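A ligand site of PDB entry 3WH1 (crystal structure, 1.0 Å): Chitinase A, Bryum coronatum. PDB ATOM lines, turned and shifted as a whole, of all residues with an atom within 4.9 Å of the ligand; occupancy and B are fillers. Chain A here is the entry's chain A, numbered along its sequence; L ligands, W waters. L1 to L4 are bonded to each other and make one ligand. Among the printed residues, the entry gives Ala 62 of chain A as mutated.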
ATOM      1  N   GLN A  61      13.159  22.951 -17.566  1.00  0.00           N
ATOM      2  CA  GLN A  61      14.394  23.033 -16.795  1.00  0.00           C
ATOM      3  C   GLN A  61      14.604  21.808 -15.912  1.00  0.00           C
ATOM      4  O   GLN A  61      15.678  21.193 -15.929  1.00  0.00           O
ATOM      5  CB  GLN A  61      14.406  24.308 -15.927  1.00  0.00           C
ATOM      6  CG  GLN A  61      15.511  24.343 -14.870  1.00  0.00           C
ATOM      7  CD  GLN A  61      16.896  24.360 -15.470  1.00  0.00           C
ATOM      8  OE1 GLN A  61      17.075  24.716 -16.640  1.00  0.00           O
ATOM      9  NE2 GLN A  61      17.885  23.968 -14.689  1.00  0.00           N
ATOM     10  N   ALA A  62      13.585  21.470 -15.128  1.00  0.00           N
ATOM     11  CA  ALA A  62      13.722  20.420 -14.121  1.00  0.00           C
ATOM     12  C   ALA A  62      14.014  19.062 -14.731  1.00  0.00           C
ATOM     13  O   ALA A  62      14.834  18.299 -14.206  1.00  0.00           O
ATOM     14  CB  ALA A  62      12.459  20.349 -13.266  1.00  0.00           C
ATOM     15  N   SER A  63      13.330  18.757 -15.823  1.00  0.00           N
ATOM     16  CA  SER A  63      13.328  17.416 -16.391  1.00  0.00           C
ATOM     17  C   SER A  63      14.196  17.273 -17.632  1.00  0.00           C
ATOM     18  O   SER A  63      14.234  16.198 -18.225  1.00  0.00           O
ATOM     19  CB  SER A  63      11.899  17.000 -16.731  1.00  0.00           C
ATOM     20  OG  SER A  63      11.409  17.747 -17.835  1.00  0.00           O
ATOM     21  N   GLY A  64      14.883  18.340 -18.020  1.00  0.00           N
ATOM     22  CA  GLY A  64      15.689  18.329 -19.246  1.00  0.00           C
ATOM     23  C   GLY A  64      14.839  18.072 -20.479  1.00  0.00           C
ATOM     24  O   GLY A  64      15.085  17.120 -21.227  1.00  0.00           O
ATOM     25  N   PHE A  68      14.127  13.162 -18.771  1.00  0.00           N
ATOM     26  CA  PHE A  68      14.402  12.415 -17.557  1.00  0.00           C
ATOM     27  C   PHE A  68      13.190  12.283 -16.661  1.00  0.00           C
ATOM     28  O   PHE A  68      12.416  13.232 -16.482  1.00  0.00           O
ATOM     29  CB  PHE A  68      15.569  13.052 -16.809  1.00  0.00           C
ATOM     30  CG  PHE A  68      16.831  13.058 -17.613  1.00  0.00           C
ATOM     31  CD1 PHE A  68      17.520  11.870 -17.846  1.00  0.00           C
ATOM     32  CD2 PHE A  68      17.319  14.235 -18.164  1.00  0.00           C
ATOM     33  CE1 PHE A  68      18.682  11.856 -18.609  1.00  0.00           C
ATOM     34  CE2 PHE A  68      18.481  14.235 -18.929  1.00  0.00           C
ATOM     35  CZ  PHE A  68      19.167  13.049 -19.147  1.00  0.00           C
ATOM     36  N   GLN A  70      13.767  10.463 -13.527  1.00  0.00           N
ATOM     37  CA  GLN A  70      14.427  10.486 -12.238  1.00  0.00           C
ATOM     38  C   GLN A  70      15.580  11.470 -12.255  1.00  0.00           C
ATOM     39  O   GLN A  70      16.248  11.644 -13.285  1.00  0.00           O
ATOM     40  CB  GLN A  70      14.981   9.090 -11.912  1.00  0.00           C
ATOM     41  CG  GLN A  70      13.942   7.985 -11.915  1.00  0.00           C
ATOM     42  CD  GLN A  70      14.524   6.646 -11.526  1.00  0.00           C
ATOM     43  OE1 GLN A  70      14.796   6.378 -10.357  1.00  0.00           O
ATOM     44  NE2 GLN A  70      14.708   5.775 -12.522  1.00  0.00           N
ATOM     45  N   GLU A  71      15.840  12.091 -11.104  1.00  0.00           N
ATOM     46  CA  GLU A  71      17.022  12.912 -10.922  1.00  0.00           C
ATOM     47  C   GLU A  71      18.253  12.116 -11.335  1.00  0.00           C
ATOM     48  O   GLU A  71      18.394  10.949 -10.967  1.00  0.00           O
ATOM     49  CB  GLU A  71      17.143  13.306  -9.451  1.00  0.00           C
ATOM     50  CG  GLU A  71      18.310  14.242  -9.139  1.00  0.00           C
ATOM     51  CD  GLU A  71      18.343  14.672  -7.683  1.00  0.00           C
ATOM     52  OE1 GLU A  71      17.315  14.553  -6.986  1.00  0.00           O
ATOM     53  OE2 GLU A  71      19.413  15.130  -7.231  1.00  0.00           O
ATOM     54  N   GLN A  72      19.131  12.740 -12.102  1.00  0.00           N
ATOM     55  CA  GLN A  72      20.343  12.090 -12.559  1.00  0.00           C
ATOM     56  C   GLN A  72      21.445  12.243 -11.526  1.00  0.00           C
ATOM     57  O   GLN A  72      21.688  13.340 -11.011  1.00  0.00           O
ATOM     58  CB  GLN A  72      20.759  12.633 -13.931  1.00  0.00           C
ATOM     59  CG  GLN A  72      19.727  12.365 -15.017  1.00  0.00           C
ATOM     60  CD  GLN A  72      19.471  10.889 -15.241  1.00  0.00           C
ATOM     61  OE1 GLN A  72      20.312  10.179 -15.785  1.00  0.00           O
ATOM     62  NE2 GLN A  72      18.298  10.407 -14.825  1.00  0.00           N
ATOM     63  N   TYR A  78      17.376  12.253   0.317  1.00  0.00           N
ATOM     64  CA  TYR A  78      16.395  13.321   0.521  1.00  0.00           C
ATOM     65  C   TYR A  78      15.399  13.000   1.649  1.00  0.00           C
ATOM     66  O   TYR A  78      14.208  13.360   1.566  1.00  0.00           O
ATOM     67  CB  TYR A  78      15.673  13.648  -0.787  1.00  0.00           C
ATOM     68  CG  TYR A  78      16.509  14.339  -1.848  1.00  0.00           C
ATOM     69  CD1 TYR A  78      17.410  13.626  -2.641  1.00  0.00           C
ATOM     70  CD2 TYR A  78      16.338  15.706  -2.101  1.00  0.00           C
ATOM     71  CE1 TYR A  78      18.161  14.271  -3.640  1.00  0.00           C
ATOM     72  CE2 TYR A  78      17.077  16.352  -3.088  1.00  0.00           C
ATOM     73  CZ  TYR A  78      17.982  15.629  -3.851  1.00  0.00           C
ATOM     74  OH  TYR A  78      18.719  16.270  -4.830  1.00  0.00           O
ATOM     75  N   ILE A 100       8.243  17.865 -12.441  1.00  0.00           N
ATOM     76  CA  ILE A 100       8.727  18.962 -11.603  1.00  0.00           C
ATOM     77  C   ILE A 100       9.858  18.511 -10.670  1.00  0.00           C
ATOM     78  O   ILE A 100      10.327  19.279  -9.837  1.00  0.00           O
ATOM     79  CB  ILE A 100       7.552  19.634 -10.822  1.00  0.00           C
ATOM     80  CG1 ILE A 100       7.848  21.108 -10.539  1.00  0.00           C
ATOM     81  CG2 ILE A 100       7.185  18.840  -9.562  1.00  0.00           C
ATOM     82  CD1 ILE A 100       6.618  21.910 -10.133  1.00  0.00           C
ATOM     83  N   GLN A 101      10.315  17.264 -10.818  1.00  0.00           N
ATOM     84  CA  GLN A 101      11.392  16.748  -9.975  1.00  0.00           C
ATOM     85  C   GLN A 101      11.056  16.862  -8.487  1.00  0.00           C
ATOM     86  O   GLN A 101      11.842  17.351  -7.680  1.00  0.00           O
ATOM     87  CB  GLN A 101      12.730  17.414 -10.337  1.00  0.00           C
ATOM     88  CG  GLN A 101      13.219  16.994 -11.699  1.00  0.00           C
ATOM     89  CD  GLN A 101      13.717  15.584 -11.709  1.00  0.00           C
ATOM     90  OE1 GLN A 101      14.807  15.326 -11.215  1.00  0.00           O
ATOM     91  NE2 GLN A 101      12.933  14.655 -12.257  1.00  0.00           N
ATOM     92  N   LEU A 102       9.858  16.387  -8.149  1.00  0.00           N
ATOM     93  CA  LEU A 102       9.380  16.344  -6.779  1.00  0.00           C
ATOM     94  C   LEU A 102      10.436  15.691  -5.894  1.00  0.00           C
ATOM     95  O   LEU A 102      10.895  14.591  -6.197  1.00  0.00           O
ATOM     96  CB  LEU A 102       8.085  15.544  -6.696  1.00  0.00           C
ATOM     97  CG  LEU A 102       7.296  15.699  -5.390  1.00  0.00           C
ATOM     98  CD1 LEU A 102       6.511  17.007  -5.380  1.00  0.00           C
ATOM     99  CD2 LEU A 102       6.386  14.507  -5.176  1.00  0.00           C
ATOM    100  N   SER A 103      10.789  16.367  -4.797  1.00  0.00           N
ATOM    101  CA  SER A 103      11.885  15.966  -3.936  1.00  0.00           C
ATOM    102  C   SER A 103      11.484  16.130  -2.474  1.00  0.00           C
ATOM    103  O   SER A 103      10.687  17.006  -2.137  1.00  0.00           O
ATOM    104  CB  SER A 103      13.106  16.847  -4.203  1.00  0.00           C
ATOM    105  OG  SER A 103      13.565  16.724  -5.541  1.00  0.00           O
ATOM    106  N   TRP A 104      12.065  15.264  -1.628  1.00  0.00           N
ATOM    107  CA  TRP A 104      11.995  15.324  -0.153  1.00  0.00           C
ATOM    108  C   TRP A 104      10.776  14.621   0.426  1.00  0.00           C
ATOM    109  O   TRP A 104       9.671  14.718  -0.109  1.00  0.00           O
ATOM    110  CB  TRP A 104      12.061  16.754   0.409  1.00  0.00           C
ATOM    111  CG  TRP A 104      13.327  17.465   0.107  1.00  0.00           C
ATOM    112  CD1 TRP A 104      13.539  18.390  -0.874  1.00  0.00           C
ATOM    113  CD2 TRP A 104      14.576  17.315   0.786  1.00  0.00           C
ATOM    114  NE1 TRP A 104      14.846  18.825  -0.843  1.00  0.00           N
ATOM    115  CE2 TRP A 104      15.508  18.168   0.175  1.00  0.00           C
ATOM    116  CE3 TRP A 104      14.999  16.525   1.867  1.00  0.00           C
ATOM    117  CZ2 TRP A 104      16.841  18.271   0.607  1.00  0.00           C
ATOM    118  CZ3 TRP A 104      16.323  16.621   2.292  1.00  0.00           C
ATOM    119  CH2 TRP A 104      17.220  17.487   1.657  1.00  0.00           C
ATOM    120  N   TYR A 106       8.942  15.480   2.840  1.00  0.00           N
ATOM    121  CA  TYR A 106       7.837  16.379   3.142  1.00  0.00           C
ATOM    122  C   TYR A 106       6.938  16.669   1.948  1.00  0.00           C
ATOM    123  O   TYR A 106       5.734  16.844   2.117  1.00  0.00           O
ATOM    124  CB  TYR A 106       8.308  17.684   3.807  1.00  0.00           C
ATOM    125  CG  TYR A 106       9.527  18.350   3.225  1.00  0.00           C
ATOM    126  CD1 TYR A 106      10.779  18.129   3.783  1.00  0.00           C
ATOM    127  CD2 TYR A 106       9.429  19.258   2.164  1.00  0.00           C
ATOM    128  CE1 TYR A 106      11.917  18.775   3.296  1.00  0.00           C
ATOM    129  CE2 TYR A 106      10.558  19.917   1.674  1.00  0.00           C
ATOM    130  CZ  TYR A 106      11.796  19.670   2.247  1.00  0.00           C
ATOM    131  OH  TYR A 106      12.921  20.325   1.778  1.00  0.00           O
ATOM    132  N   ASN A 107       7.515  16.685   0.746  1.00  0.00           N
ATOM    133  CA  ASN A 107       6.699  16.870  -0.462  1.00  0.00           C
ATOM    134  C   ASN A 107       6.010  15.593  -0.905  1.00  0.00           C
ATOM    135  O   ASN A 107       4.838  15.621  -1.263  1.00  0.00           O
ATOM    136  CB  ASN A 107       7.510  17.460  -1.609  1.00  0.00           C
ATOM    137  CG  ASN A 107       7.823  18.930  -1.416  1.00  0.00           C
ATOM    138  OD1 ASN A 107       7.025  19.701  -0.878  1.00  0.00           O
ATOM    139  ND2 ASN A 107       8.992  19.328  -1.874  1.00  0.00           N
ATOM    140  N   PHE A 140       1.968  20.153  -6.871  1.00  0.00           N
ATOM    141  CA  PHE A 140       2.933  21.084  -6.309  1.00  0.00           C
ATOM    142  C   PHE A 140       2.589  22.506  -6.763  1.00  0.00           C
ATOM    143  O   PHE A 140       2.537  23.442  -5.960  1.00  0.00           O
ATOM    144  CB  PHE A 140       4.362  20.709  -6.706  1.00  0.00           C
ATOM    145  CG  PHE A 140       5.412  21.530  -6.019  1.00  0.00           C
ATOM    146  CD1 PHE A 140       5.732  22.802  -6.491  1.00  0.00           C
ATOM    147  CD2 PHE A 140       6.053  21.066  -4.877  1.00  0.00           C
ATOM    148  CE1 PHE A 140       6.676  23.580  -5.834  1.00  0.00           C
ATOM    149  CE2 PHE A 140       7.006  21.845  -4.218  1.00  0.00           C
ATOM    150  CZ  PHE A 140       7.318  23.101  -4.704  1.00  0.00           C
ATOM    151  N   ILE A 163       9.250  29.457  -5.188  1.00  0.00           N
ATOM    152  CA  ILE A 163       8.500  28.386  -4.543  1.00  0.00           C
ATOM    153  C   ILE A 163       9.089  27.017  -4.904  1.00  0.00           C
ATOM    154  O   ILE A 163       9.228  26.142  -4.042  1.00  0.00           O
ATOM    155  CB  ILE A 163       6.998  28.502  -4.927  1.00  0.00           C
ATOM    156  CG1 ILE A 163       6.402  29.778  -4.332  1.00  0.00           C
ATOM    157  CG2 ILE A 163       6.230  27.270  -4.455  1.00  0.00           C
ATOM    158  CD1 ILE A 163       5.085  30.194  -4.955  1.00  0.00           C
ATOM    159  N   ILE A 164       9.459  26.828  -6.158  1.00  0.00           N
ATOM    160  CA  ILE A 164       9.959  25.535  -6.632  1.00  0.00           C
ATOM    161  C   ILE A 164      11.358  25.204  -6.105  1.00  0.00           C
ATOM    162  O   ILE A 164      11.609  24.068  -5.675  1.00  0.00           O
ATOM    163  CB  ILE A 164       9.921  25.479  -8.180  1.00  0.00           C
ATOM    164  CG1 ILE A 164       8.465  25.432  -8.658  1.00  0.00           C
ATOM    165  CG2 ILE A 164      10.690  24.281  -8.714  1.00  0.00           C
ATOM    166  CD1 ILE A 164       8.294  25.726 -10.122  1.00  0.00           C
ATOM    167  N   ASN A 165      12.268  26.168  -6.138  1.00  0.00           N
ATOM    168  CA  ASN A 165      13.664  25.902  -5.793  1.00  0.00           C
ATOM    169  C   ASN A 165      14.440  27.143  -5.387  1.00  0.00           C
ATOM    170  O   ASN A 165      15.626  27.266  -5.697  1.00  0.00           O
ATOM    171  CB  ASN A 165      14.371  25.163  -6.949  1.00  0.00           C
ATOM    172  CG  ASN A 165      15.604  24.374  -6.499  1.00  0.00           C
ATOM    173  OD1 ASN A 165      15.655  23.890  -5.369  1.00  0.00           O
ATOM    174  ND2 ASN A 165      16.574  24.239  -7.387  1.00  0.00           N
ATOM    175  N   LEU A 168      18.117  27.436  -3.600  1.00  0.00           N
ATOM    176  CA  LEU A 168      19.283  27.102  -4.410  1.00  0.00           C
ATOM    177  C   LEU A 168      19.439  27.939  -5.681  1.00  0.00           C
ATOM    178  O   LEU A 168      20.551  28.071  -6.182  1.00  0.00           O
ATOM    179  CB  LEU A 168      19.276  25.608  -4.764  1.00  0.00           C
ATOM    180  CG  LEU A 168      19.451  24.663  -3.574  1.00  0.00           C
ATOM    181  CD1 LEU A 168      19.212  23.222  -3.988  1.00  0.00           C
ATOM    182  CD2 LEU A 168      20.835  24.816  -2.935  1.00  0.00           C
ATOM    183  N   GLU A 169      18.344  28.511  -6.171  1.00  0.00           N
ATOM    184  CA  GLU A 169      18.380  29.200  -7.469  1.00  0.00           C
ATOM    185  C   GLU A 169      18.184  30.702  -7.425  1.00  0.00           C
ATOM    186  O   GLU A 169      18.603  31.413  -8.338  1.00  0.00           O
ATOM    187  CB  GLU A 169      17.391  28.572  -8.444  1.00  0.00           C
ATOM    188  CG  GLU A 169      17.764  27.156  -8.848  1.00  0.00           C
ATOM    189  CD  GLU A 169      16.871  26.610  -9.944  1.00  0.00           C
ATOM    190  OE1 GLU A 169      16.391  27.386 -10.789  1.00  0.00           O
ATOM    191  OE2 GLU A 169      16.669  25.384  -9.956  1.00  0.00           O
ATOM    192  N   ILE A 177      26.042  28.464 -10.656  1.00  0.00           N
ATOM    193  CA  ILE A 177      25.220  27.375 -11.184  1.00  0.00           C
ATOM    194  C   ILE A 177      23.721  27.567 -10.909  1.00  0.00           C
ATOM    195  O   ILE A 177      22.896  27.391 -11.798  1.00  0.00           O
ATOM    196  CB  ILE A 177      25.717  25.961 -10.730  1.00  0.00           C
ATOM    197  CG1 ILE A 177      24.958  24.852 -11.469  1.00  0.00           C
ATOM    198  CG2 ILE A 177      25.624  25.777  -9.208  1.00  0.00           C
ATOM    199  CD1 ILE A 177      25.253  24.768 -12.954  1.00  0.00           C
ATOM    200  N   MET A 180      22.369  30.290 -13.096  1.00  0.00           N
ATOM    201  CA  MET A 180      22.238  29.822 -14.473  1.00  0.00           C
ATOM    202  C   MET A 180      20.996  28.946 -14.661  1.00  0.00           C
ATOM    203  O   MET A 180      20.314  29.033 -15.685  1.00  0.00           O
ATOM    204  CB  MET A 180      23.502  29.111 -14.941  1.00  0.00           C
ATOM    205  CG  MET A 180      24.686  30.066 -15.014  1.00  0.00           C
ATOM    206  SD  MET A 180      26.178  29.364 -15.699  1.00  0.00           S
ATOM    207  CE  MET A 180      25.739  29.301 -17.441  1.00  0.00           C
ATOM    208  N   GLN A 181      20.700  28.119 -13.658  1.00  0.00           N
ATOM    209  CA  GLN A 181      19.463  27.321 -13.666  1.00  0.00           C
ATOM    210  C   GLN A 181      18.236  28.239 -13.674  1.00  0.00           C
ATOM    211  O   GLN A 181      17.308  28.043 -14.457  1.00  0.00           O
ATOM    212  CB  GLN A 181      19.441  26.378 -12.465  1.00  0.00           C
ATOM    213  CG  GLN A 181      20.483  25.277 -12.566  1.00  0.00           C
ATOM    214  CD  GLN A 181      20.780  24.575 -11.258  1.00  0.00           C
ATOM    215  OE1 GLN A 181      20.605  25.128 -10.178  1.00  0.00           O
ATOM    216  NE2 GLN A 181      21.290  23.353 -11.362  1.00  0.00           N
ATOM    217  N   ASN A 184      17.831  29.885 -17.014  1.00  0.00           N
ATOM    218  CA  ASN A 184      17.275  28.947 -17.988  1.00  0.00           C
ATOM    219  C   ASN A 184      15.768  28.809 -17.862  1.00  0.00           C
ATOM    220  O   ASN A 184      15.072  28.792 -18.869  1.00  0.00           O
ATOM    221  CB  ASN A 184      17.986  27.606 -17.936  1.00  0.00           C
ATOM    222  CG  ASN A 184      19.392  27.665 -18.537  1.00  0.00           C
ATOM    223  OD1 ASN A 184      19.685  28.526 -19.369  1.00  0.00           O
ATOM    224  ND2 ASN A 184      20.248  26.762 -18.103  1.00  0.00           N
ATOM    225  N   ARG A 185      15.236  28.752 -16.632  1.00  0.00           N
ATOM    226  CA  ARG A 185      13.790  28.762 -16.439  1.00  0.00           C
ATOM    227  C   ARG A 185      13.162  29.976 -17.120  1.00  0.00           C
ATOM    228  O   ARG A 185      12.145  29.860 -17.808  1.00  0.00           O
ATOM    229  CB  ARG A 185      13.424  28.777 -14.960  1.00  0.00           C
ATOM    230  CG  ARG A 185      13.871  27.558 -14.191  1.00  0.00           C
ATOM    231  CD  ARG A 185      13.549  27.735 -12.715  1.00  0.00           C
ATOM    232  NE  ARG A 185      14.094  26.644 -11.914  1.00  0.00           N
ATOM    233  CZ  ARG A 185      13.495  25.465 -11.726  1.00  0.00           C
ATOM    234  NH1 ARG A 185      12.311  25.216 -12.256  1.00  0.00           N
ATOM    235  NH2 ARG A 185      14.097  24.549 -10.993  1.00  0.00           N
HETATM  236  C1  LIG L   1      20.738  20.864 -17.241  1.00  0.00           C
HETATM  237  C2  LIG L   1      20.512  21.828 -16.076  1.00  0.00           C
HETATM  238  C3  LIG L   1      20.312  21.045 -14.784  1.00  0.00           C
HETATM  239  C4  LIG L   1      19.195  19.995 -14.955  1.00  0.00           C
HETATM  240  C5  LIG L   1      19.459  19.135 -16.198  1.00  0.00           C
HETATM  241  C6  LIG L   1      18.286  18.202 -16.481  1.00  0.00           C
HETATM  242  C7  LIG L   1      21.418  24.097 -15.974  1.00  0.00           C
HETATM  243  C8  LIG L   1      22.636  24.956 -15.818  1.00  0.00           C
HETATM  244  N1  LIG L   1      21.612  22.783 -15.933  1.00  0.00           N
HETATM  245  O1  LIG L   1      20.795  21.615 -18.433  1.00  0.00           O
HETATM  246  O2  LIG L   1      20.009  21.960 -13.752  1.00  0.00           O
HETATM  247  O3  LIG L   1      19.142  19.120 -13.848  1.00  0.00           O
HETATM  248  O4  LIG L   1      19.670  19.942 -17.338  1.00  0.00           O
HETATM  249  O5  LIG L   1      18.631  17.261 -17.473  1.00  0.00           O
HETATM  250  O6  LIG L   1      20.315  24.630 -16.120  1.00  0.00           O
HETATM  251  C1  LG2 L   2      18.075  19.465 -12.969  1.00  0.00           C
HETATM  252  C2  LG2 L   2      17.752  18.222 -12.124  1.00  0.00           C
HETATM  253  C3  LG2 L   2      16.797  18.599 -10.987  1.00  0.00           C
HETATM  254  C4  LG2 L   2      17.234  19.907 -10.300  1.00  0.00           C
HETATM  255  C5  LG2 L   2      17.475  21.013 -11.311  1.00  0.00           C
HETATM  256  C6  LG2 L   2      17.908  22.347 -10.708  1.00  0.00           C
HETATM  257  C7  LG2 L   2      17.579  16.020 -13.236  1.00  0.00           C
HETATM  258  C8  LG2 L   2      16.757  15.223 -14.193  1.00  0.00           C
HETATM  259  N1  LG2 L   2      17.136  17.255 -13.004  1.00  0.00           N
HETATM  260  O1  LG2 L   2      16.646  17.480 -10.123  1.00  0.00           O
HETATM  261  O2  LG2 L   2      16.236  20.506  -9.540  1.00  0.00           O
HETATM  262  O3  LG2 L   2      18.470  20.571 -12.193  1.00  0.00           O
HETATM  263  O4  LG2 L   2      17.729  23.377 -11.662  1.00  0.00           O
HETATM  264  O5  LG2 L   2      18.577  15.521 -12.708  1.00  0.00           O
HETATM  265  C1  LG3 L   3      15.930  19.939  -8.267  1.00  0.00           C
HETATM  266  C2  LG3 L   3      16.582  20.693  -7.121  1.00  0.00           C
HETATM  267  C3  LG3 L   3      15.845  20.441  -5.805  1.00  0.00           C
HETATM  268  C4  LG3 L   3      14.378  20.750  -5.988  1.00  0.00           C
HETATM  269  C5  LG3 L   3      13.875  19.928  -7.169  1.00  0.00           C
HETATM  270  C6  LG3 L   3      12.439  20.247  -7.507  1.00  0.00           C
HETATM  271  C7  LG3 L   3      18.976  21.230  -7.062  1.00  0.00           C
HETATM  272  C8  LG3 L   3      20.352  20.671  -6.852  1.00  0.00           C
HETATM  273  N1  LG3 L   3      17.990  20.349  -6.952  1.00  0.00           N
HETATM  274  O1  LG3 L   3      16.375  21.282  -4.809  1.00  0.00           O
HETATM  275  O2  LG3 L   3      13.591  20.367  -4.891  1.00  0.00           O
HETATM  276  O3  LG3 L   3      14.589  20.251  -8.317  1.00  0.00           O
HETATM  277  O4  LG3 L   3      12.298  21.626  -7.705  1.00  0.00           O
HETATM  278  O5  LG3 L   3      18.833  22.432  -7.312  1.00  0.00           O
HETATM  279  C1  LG4 L   4      13.192  21.461  -4.074  1.00  0.00           C
HETATM  280  C2  LG4 L   4      11.724  21.280  -3.688  1.00  0.00           C
HETATM  281  C3  LG4 L   4      11.296  22.334  -2.676  1.00  0.00           C
HETATM  282  C4  LG4 L   4      12.293  22.461  -1.529  1.00  0.00           C
HETATM  283  C5  LG4 L   4      13.718  22.577  -2.068  1.00  0.00           C
HETATM  284  C6  LG4 L   4      14.726  22.603  -0.935  1.00  0.00           C
HETATM  285  C7  LG4 L   4      10.131  20.304  -5.291  1.00  0.00           C
HETATM  286  C8  LG4 L   4       9.311  20.537  -6.527  1.00  0.00           C
HETATM  287  N1  LG4 L   4      10.858  21.343  -4.862  1.00  0.00           N
HETATM  288  O1  LG4 L   4      10.018  21.980  -2.180  1.00  0.00           O
HETATM  289  O2  LG4 L   4      11.969  23.579  -0.729  1.00  0.00           O
HETATM  290  O3  LG4 L   4      14.001  21.477  -2.914  1.00  0.00           O
HETATM  291  O4  LG4 L   4      16.025  22.819  -1.445  1.00  0.00           O
HETATM  292  O5  LG4 L   4      10.121  19.195  -4.727  1.00  0.00           O
HETATM  293  O   HOH W   1      16.226  17.030  -6.273  1.00  0.00           O
HETATM  294  O   HOH W   2      16.837  20.459  -2.344  1.00  0.00           O
HETATM  295  O   HOH W   3      11.582  21.611 -10.299  1.00  0.00           O
HETATM  296  O   HOH W   4      18.360  23.725 -18.718  1.00  0.00           O
HETATM  297  O   HOH W   5      24.228  21.831 -15.175  1.00  0.00           O
HETATM  298  O   HOH W   6      14.219  21.709 -10.930  1.00  0.00           O
HETATM  299  O   HOH W   7      20.991  15.877 -11.491  1.00  0.00           O
HETATM  300  O   HOH W   8      20.340  15.539 -16.123  1.00  0.00           O
HETATM  301  O   HOH W   9      19.493  17.974 -19.939  1.00  0.00           O
HETATM  302  O   HOH W  10      12.752  23.166   1.952  1.00  0.00           O
HETATM  303  O   HOH W  11      17.314  21.258 -18.242  1.00  0.00           O
HETATM  304  O   HOH W  12      16.053  25.165  -3.015  1.00  0.00           O
HETATM  305  O   HOH W  13      21.416  23.981 -19.496  1.00  0.00           O
HETATM  306  O   HOH W  14      11.318  25.894  -2.066  1.00  0.00           O
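O1 of LG3 L3 sits at hydrogen-bond distance from OD1 of Asn 165 (2.8 Å).
The backbone carbonyl oxygen (O) of Ala 62 sits at hydrogen-bond distance from a nitrogen (N1) of LG2 L2 (2.8 Å).
OE2 of Glu 169 lies within hydrogen-bond range of O4 of LG2 L2, 2.8 Å away.
ND2 of Asn 107 lies within hydrogen-bond range of O1 of LG4 L4 (2.9 Å).
NE2 of Gln 61 lies within hydrogen-bond range of O6 of LIG L1, at 2.9 Å.
N of Gln 72 sits at hydrogen-bond distance from O5 of LG2 L2, 2.9 Å away.
The backbone NH (N) of Ser 103 lies within hydrogen-bond range of an oxygen (O5) of LG4 L4, at 2.9 Å.
The side-chain amide nitrogen (ND2) of Asn 184 lies within hydrogen-bond range of an oxygen (O6) of LIG L1 (2.9 Å).
The backbone carbonyl oxygen of Ile 164 lies within hydrogen-bond range of a nitrogen (N1) of LG4 L4 (2.9 Å).
OE1 of Gln 101 lies within hydrogen-bond range of O1 of LG2 L2, at 3.0 Å.
O2 of LIG L1 is in hydrogen-bond range of NE2 of Gln 181, at 3.0 Å.
O3 of LG4 L4 is in hydrogen-bond range of NE1 of Trp 104 (3.5 Å).
ND2 of Asn 165 sits at hydrogen-bond distance from OE2 of Glu 169, at 2.8 Å.
The side-chain carboxylate (OE1) of Glu 169 lies within salt-bridge range of the guanidinium group (NE) of Arg 185.
The backbone carbonyl oxygen of Ser 103 lies within hydrogen-bond range of the side-chain amide nitrogen of Asn 107 (2.9 Å).
The side-chain amide nitrogen (NE2) of Gln 72 is in hydrogen-bond range of the backbone carbonyl oxygen (O) of Gln 70, at 2.8 Å.
O of Gln 101 is in hydrogen-bond range of OG of Ser 103, 2.8 Å away.
The backbone carbonyl oxygen (O) of Met 180 sits close to the side-chain amide nitrogen (ND2) of Asn 184 (3.3 Å).
N of Phe 68 lies within hydrogen-bond range of O of Ser 63 (3.1 Å).
The side-chain carboxylate of Glu 71 sits at hydrogen-bond distance from the side-chain hydroxyl of Tyr 78 (2.7 Å).
Residues that only touch the ligand: Gly 64 (3.6 Å), Phe 68 (3.4 Å), Gln 70 (3.7 Å), Glu 71 (3.5 Å), Ile 100 (3.3 Å), Leu 102 (3.6 Å), Tyr 106 (3.98 Å), Phe 140 (3.5 Å), Leu 168 (3.4 Å), Ile 177 (3.9 Å) and Arg 185 (3.9 Å).
Of the 27 residues printed, 23 come within 4 Å of the ligand.
The nearest printed residue that does not touch the ligand is Met 180 (4.3 Å).
Water W2 bridges an oxygen (O1) of LG3 L3 (2.6 Å) and the indole nitrogen of Trp 104 (3.0 Å).
Water W3 lies within hydrogen-bond range of O of Ile 100 (2.7 Å) and O4 of LG3 L3 (2.7 Å).
Water W7 lies within hydrogen-bond range of O of Gln 72 (2.7 Å) and O5 of LG2 L2 (2.7 Å).
Water W14 bridges an oxygen (O2) of LG4 L4 and the backbone carbonyl oxygen (O) of Ile 163.
Water W11 bridges the backbone carbonyl oxygen (O) of Gln 61 and an oxygen (O4) of LIG L1.
Water W4 bridges the side-chain amide oxygen (OE1) of Gln 61 (2.6 Å) and an oxygen (O1) of LIG L1 (3.2 Å).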
